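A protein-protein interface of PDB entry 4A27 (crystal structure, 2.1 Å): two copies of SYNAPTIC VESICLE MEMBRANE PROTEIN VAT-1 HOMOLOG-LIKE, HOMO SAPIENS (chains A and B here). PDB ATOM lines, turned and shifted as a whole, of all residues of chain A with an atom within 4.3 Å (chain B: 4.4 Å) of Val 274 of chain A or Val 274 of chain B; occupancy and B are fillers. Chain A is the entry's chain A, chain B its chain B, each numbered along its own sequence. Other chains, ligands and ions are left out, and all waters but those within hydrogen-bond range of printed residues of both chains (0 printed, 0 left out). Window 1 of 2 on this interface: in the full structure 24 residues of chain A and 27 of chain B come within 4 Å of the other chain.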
ATOM      1  N   VAL A 137      -7.506   9.020 -13.208  1.00  0.00           N
ATOM      2  CA  VAL A 137      -7.367   8.511 -11.850  1.00  0.00           C
ATOM      3  C   VAL A 137      -5.974   8.893 -11.316  1.00  0.00           C
ATOM      4  O   VAL A 137      -5.846   9.706 -10.409  1.00  0.00           O
ATOM      5  CB  VAL A 137      -7.636   7.009 -11.778  1.00  0.00           C
ATOM      6  CG1 VAL A 137      -7.430   6.525 -10.374  1.00  0.00           C
ATOM      7  CG2 VAL A 137      -9.053   6.708 -12.271  1.00  0.00           C
ATOM      8  N   GLY A 232       2.282   7.641  -4.428  1.00  0.00           N
ATOM      9  CA  GLY A 232       1.911   6.767  -5.530  1.00  0.00           C
ATOM     10  C   GLY A 232       0.473   6.281  -5.492  1.00  0.00           C
ATOM     11  O   GLY A 232      -0.167   6.301  -4.443  1.00  0.00           O
ATOM     12  N   THR A 233       0.004   5.753  -6.633  1.00  0.00           N
ATOM     13  CA  THR A 233      -1.410   5.336  -6.829  1.00  0.00           C
ATOM     14  C   THR A 233      -1.467   3.888  -7.301  1.00  0.00           C
ATOM     15  O   THR A 233      -0.815   3.509  -8.269  1.00  0.00           O
ATOM     16  CB  THR A 233      -2.114   6.170  -7.910  1.00  0.00           C
ATOM     17  OG1 THR A 233      -2.023   7.564  -7.588  1.00  0.00           O
ATOM     18  CG2 THR A 233      -3.580   5.769  -8.038  1.00  0.00           C
ATOM     19  N   TYR A 234      -2.199   3.075  -6.562  1.00  0.00           N
ATOM     20  CA  TYR A 234      -2.488   1.719  -6.955  1.00  0.00           C
ATOM     21  C   TYR A 234      -3.928   1.689  -7.486  1.00  0.00           C
ATOM     22  O   TYR A 234      -4.831   2.170  -6.815  1.00  0.00           O
ATOM     23  CB  TYR A 234      -2.292   0.801  -5.736  1.00  0.00           C
ATOM     24  CG  TYR A 234      -2.578  -0.649  -5.984  1.00  0.00           C
ATOM     25  CD1 TYR A 234      -1.604  -1.507  -6.468  1.00  0.00           C
ATOM     26  CD2 TYR A 234      -3.814  -1.173  -5.670  1.00  0.00           C
ATOM     27  CE1 TYR A 234      -1.875  -2.840  -6.676  1.00  0.00           C
ATOM     28  CE2 TYR A 234      -4.085  -2.499  -5.851  1.00  0.00           C
ATOM     29  CZ  TYR A 234      -3.122  -3.327  -6.366  1.00  0.00           C
ATOM     30  OH  TYR A 234      -3.432  -4.646  -6.553  1.00  0.00           O
ATOM     31  N   LYS A 273      -0.202   7.054   0.582  1.00  0.00           N
ATOM     32  CA  LYS A 273      -0.565   6.350  -0.639  1.00  0.00           C
ATOM     33  C   LYS A 273      -2.050   6.450  -0.996  1.00  0.00           C
ATOM     34  O   LYS A 273      -2.872   6.837  -0.170  1.00  0.00           O
ATOM     35  CB  LYS A 273      -0.107   4.913  -0.517  1.00  0.00           C
ATOM     36  CG  LYS A 273       1.389   4.777  -0.788  1.00  0.00           C
ATOM     37  CD  LYS A 273       1.981   3.520  -0.158  1.00  0.00           C
ATOM     38  CE  LYS A 273       3.532   3.544  -0.218  1.00  0.00           C
ATOM     39  NZ  LYS A 273       4.162   2.191   0.068  1.00  0.00           N
ATOM     40  N   VAL A 274      -2.314   6.162  -2.267  1.00  0.00           N
ATOM     41  CA  VAL A 274      -3.579   6.321  -2.936  1.00  0.00           C
ATOM     42  C   VAL A 274      -4.003   4.958  -3.470  1.00  0.00           C
ATOM     43  O   VAL A 274      -3.229   4.262  -4.130  1.00  0.00           O
ATOM     44  CB  VAL A 274      -3.428   7.259  -4.161  1.00  0.00           C
ATOM     45  CG1 VAL A 274      -4.760   7.564  -4.787  1.00  0.00           C
ATOM     46  CG2 VAL A 274      -2.742   8.538  -3.756  1.00  0.00           C
ATOM     47  N   ILE A 275      -5.252   4.590  -3.201  1.00  0.00           N
ATOM     48  CA  ILE A 275      -5.837   3.403  -3.793  1.00  0.00           C
ATOM     49  C   ILE A 275      -7.101   3.759  -4.507  1.00  0.00           C
ATOM     50  O   ILE A 275      -7.925   4.467  -3.963  1.00  0.00           O
ATOM     51  CB  ILE A 275      -6.161   2.401  -2.724  1.00  0.00           C
ATOM     52  CG1 ILE A 275      -4.854   1.925  -2.086  1.00  0.00           C
ATOM     53  CG2 ILE A 275      -6.908   1.201  -3.325  1.00  0.00           C
ATOM     54  CD1 ILE A 275      -5.033   1.270  -0.697  1.00  0.00           C
ATOM     55  N   ALA A 276      -7.268   3.208  -5.703  1.00  0.00           N
ATOM     56  CA  ALA A 276      -8.401   3.486  -6.552  1.00  0.00           C
ATOM     57  C   ALA A 276      -8.913   2.201  -7.186  1.00  0.00           C
ATOM     58  O   ALA A 276      -8.173   1.232  -7.359  1.00  0.00           O
ATOM     59  CB  ALA A 276      -8.000   4.452  -7.646  1.00  0.00           C
ATOM     60  N   VAL B 137      -2.240  14.882  -4.738  1.00  0.00           N
ATOM     61  CA  VAL B 137      -3.048  13.707  -4.456  1.00  0.00           C
ATOM     62  C   VAL B 137      -4.268  13.732  -5.385  1.00  0.00           C
ATOM     63  O   VAL B 137      -4.366  12.927  -6.285  1.00  0.00           O
ATOM     64  CB  VAL B 137      -3.396  13.629  -2.956  1.00  0.00           C
ATOM     65  CG1 VAL B 137      -4.216  12.373  -2.624  1.00  0.00           C
ATOM     66  CG2 VAL B 137      -2.131  13.632  -2.151  1.00  0.00           C
ATOM     67  N   GLY B 232     -14.205  10.539  -8.053  1.00  0.00           N
ATOM     68  CA  GLY B 232     -13.858  11.454  -6.990  1.00  0.00           C
ATOM     69  C   GLY B 232     -12.858  10.888  -6.022  1.00  0.00           C
ATOM     70  O   GLY B 232     -12.585   9.683  -6.017  1.00  0.00           O
ATOM     71  N   THR B 233     -12.330  11.761  -5.168  1.00  0.00           N
ATOM     72  CA  THR B 233     -11.267  11.385  -4.247  1.00  0.00           C
ATOM     73  C   THR B 233     -11.559  11.823  -2.845  1.00  0.00           C
ATOM     74  O   THR B 233     -11.819  12.984  -2.588  1.00  0.00           O
ATOM     75  CB  THR B 233      -9.911  12.043  -4.658  1.00  0.00           C
ATOM     76  OG1 THR B 233      -9.598  11.683  -6.003  1.00  0.00           O
ATOM     77  CG2 THR B 233      -8.799  11.555  -3.733  1.00  0.00           C
ATOM     78  N   TYR B 234     -11.426  10.883  -1.931  1.00  0.00           N
ATOM     79  CA  TYR B 234     -11.520  11.142  -0.525  1.00  0.00           C
ATOM     80  C   TYR B 234     -10.103  11.073   0.079  1.00  0.00           C
ATOM     81  O   TYR B 234      -9.394  10.118  -0.129  1.00  0.00           O
ATOM     82  CB  TYR B 234     -12.458  10.102   0.084  1.00  0.00           C
ATOM     83  CG  TYR B 234     -12.643  10.233   1.560  1.00  0.00           C
ATOM     84  CD1 TYR B 234     -13.619  11.064   2.094  1.00  0.00           C
ATOM     85  CD2 TYR B 234     -11.851   9.505   2.438  1.00  0.00           C
ATOM     86  CE1 TYR B 234     -13.782  11.175   3.479  1.00  0.00           C
ATOM     87  CE2 TYR B 234     -12.010   9.608   3.803  1.00  0.00           C
ATOM     88  CZ  TYR B 234     -12.969  10.438   4.316  1.00  0.00           C
ATOM     89  OH  TYR B 234     -13.105  10.506   5.677  1.00  0.00           O
ATOM     90  N   LYS B 273     -14.114   5.102  -7.349  1.00  0.00           N
ATOM     91  CA  LYS B 273     -13.626   6.071  -6.393  1.00  0.00           C
ATOM     92  C   LYS B 273     -12.180   5.825  -5.939  1.00  0.00           C
ATOM     93  O   LYS B 273     -11.634   4.753  -6.115  1.00  0.00           O
ATOM     94  CB  LYS B 273     -14.594   6.165  -5.218  1.00  0.00           C
ATOM     95  CG  LYS B 273     -15.829   6.994  -5.592  1.00  0.00           C
ATOM     96  CD  LYS B 273     -17.026   6.652  -4.748  1.00  0.00           C
ATOM     97  CE  LYS B 273     -18.309   7.286  -5.295  1.00  0.00           C
ATOM     98  NZ  LYS B 273     -19.398   7.254  -4.257  1.00  0.00           N
ATOM     99  N   VAL B 274     -11.598   6.870  -5.361  1.00  0.00           N
ATOM    100  CA  VAL B 274     -10.198   6.928  -4.967  1.00  0.00           C
ATOM    101  C   VAL B 274     -10.112   7.326  -3.509  1.00  0.00           C
ATOM    102  O   VAL B 274     -10.711   8.327  -3.099  1.00  0.00           O
ATOM    103  CB  VAL B 274      -9.528   8.002  -5.839  1.00  0.00           C
ATOM    104  CG1 VAL B 274      -7.985   8.079  -5.625  1.00  0.00           C
ATOM    105  CG2 VAL B 274      -9.891   7.688  -7.293  1.00  0.00           C
ATOM    106  N   ILE B 275      -9.363   6.566  -2.724  1.00  0.00           N
ATOM    107  CA  ILE B 275      -9.116   6.908  -1.323  1.00  0.00           C
ATOM    108  C   ILE B 275      -7.625   7.053  -1.075  1.00  0.00           C
ATOM    109  O   ILE B 275      -6.827   6.212  -1.511  1.00  0.00           O
ATOM    110  CB  ILE B 275      -9.696   5.846  -0.316  1.00  0.00           C
ATOM    111  CG1 ILE B 275      -9.345   6.227   1.121  1.00  0.00           C
ATOM    112  CG2 ILE B 275      -9.134   4.484  -0.586  1.00  0.00           C
ATOM    113  CD1 ILE B 275     -10.297   5.649   2.191  1.00  0.00           C
ATOM    114  N   ALA B 276      -7.269   8.086  -0.310  1.00  0.00           N
ATOM    115  CA  ALA B 276      -5.879   8.476  -0.111  1.00  0.00           C
ATOM    116  C   ALA B 276      -5.692   8.968   1.311  1.00  0.00           C
ATOM    117  O   ALA B 276      -6.639   9.400   1.979  1.00  0.00           O
ATOM    118  CB  ALA B 276      -5.482   9.605  -1.100  1.00  0.00           C
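The backbone NH (N) of Ile 275 of chain A sits at hydrogen-bond distance from the backbone carbonyl oxygen (O) of Ile 275 of chain B.
The backbone carbonyl oxygen (O) of Gly 232 of chain A lies within hydrogen-bond range of the backbone NH (N) of Val 274 of chain A, 3.1 Å away. The backbone carbonyl oxygen (O) of Tyr 234 of chain A sits at hydrogen-bond distance from the backbone NH (N) of Ala 276 of chain A, at 2.9 Å. The backbone NH (N) of Tyr 234 of chain A lies within hydrogen-bond range of the backbone carbonyl oxygen (O) of Val 274 of chain A, at 2.9 Å. O of Tyr 234 of chain B lies within hydrogen-bond range of N of Ala 276 of chain B (2.9 Å). O of Gly 232 of chain B sits at hydrogen-bond distance from N of Val 274 of chain B, 3.1 Å away. The backbone carbonyl oxygen (O) of Val 274 of chain B sits at hydrogen-bond distance from the backbone NH (N) of Tyr 234 of chain B (2.9 Å).
Of the 8 printed residues of chain B, 4 touch a printed residue of chain A. Of the 8 printed residues of chain A, 4 touch a printed residue of chain B. Hydrophobic or aromatic side chains of chain A that line the printed part of chain B: Val 274 and Ala 276. Among the printed residues, 8 pairs touch across the chains.
Of chain A, only Val 274, Ile 275 and Ala 276 come within 4 Å of Val 274 of chain B. Of the printed residues of chain B, Ile 275 of chain A touches Val 274 and Ile 275. Of the printed residues of chain B, Lys 273 of chain A touches Ala 276. Of the printed residues of chain A, Ile 275 of chain B touches Val 274 (3.5 Å) and Ile 275 (2.8 Å). The nearest residue of chain B that does not touch Val 274 of chain A is Val 137 of chain B (4.3 Å).
Lys 273 of chain A touches Ala 276 of chain B, and with the chains exchanged Ala 276 of chain A touches Lys 273 of chain B. Val 274 of chain A touches Ile 275 of chain B, and with the chains exchanged Ile 275 of chain A touches Val 274 of chain B. Val 274 of chain A touches Ala 276 of chain B, and with the chains exchanged Ala 276 of chain A touches Val 274 of chain B. Ile 275 of chain B touches its own counterpart, Ile 275 of chain A. Positions printed for both chains: 137, 232, 233, 234, 273, 274, 275 and 276. Of the 8 pairs that touch across the chains among the printed residues, 8 have their exchanged pair printed and touching as well.
O of Lys 273 of chain A touches CA of Ala 276 of chain B, 3.4 Å away. Val 274 of chain B touches Val 274 of chain A (CG1 to CG1, 3.4 Å). Val 274 of chain A touches Ile 275 of chain B (CA to O, 3.5 Å). Ala 276 of chain B touches Val 274 of chain A (CB to CG2, 3.96 Å). Val 274 of chain B touches Ile 275 of chain A. Ala 276 of chain A touches Lys 273 of chain B. CG2 of Val 274 of chain B touches CB of Ala 276 of chain A, 3.8 Å away.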
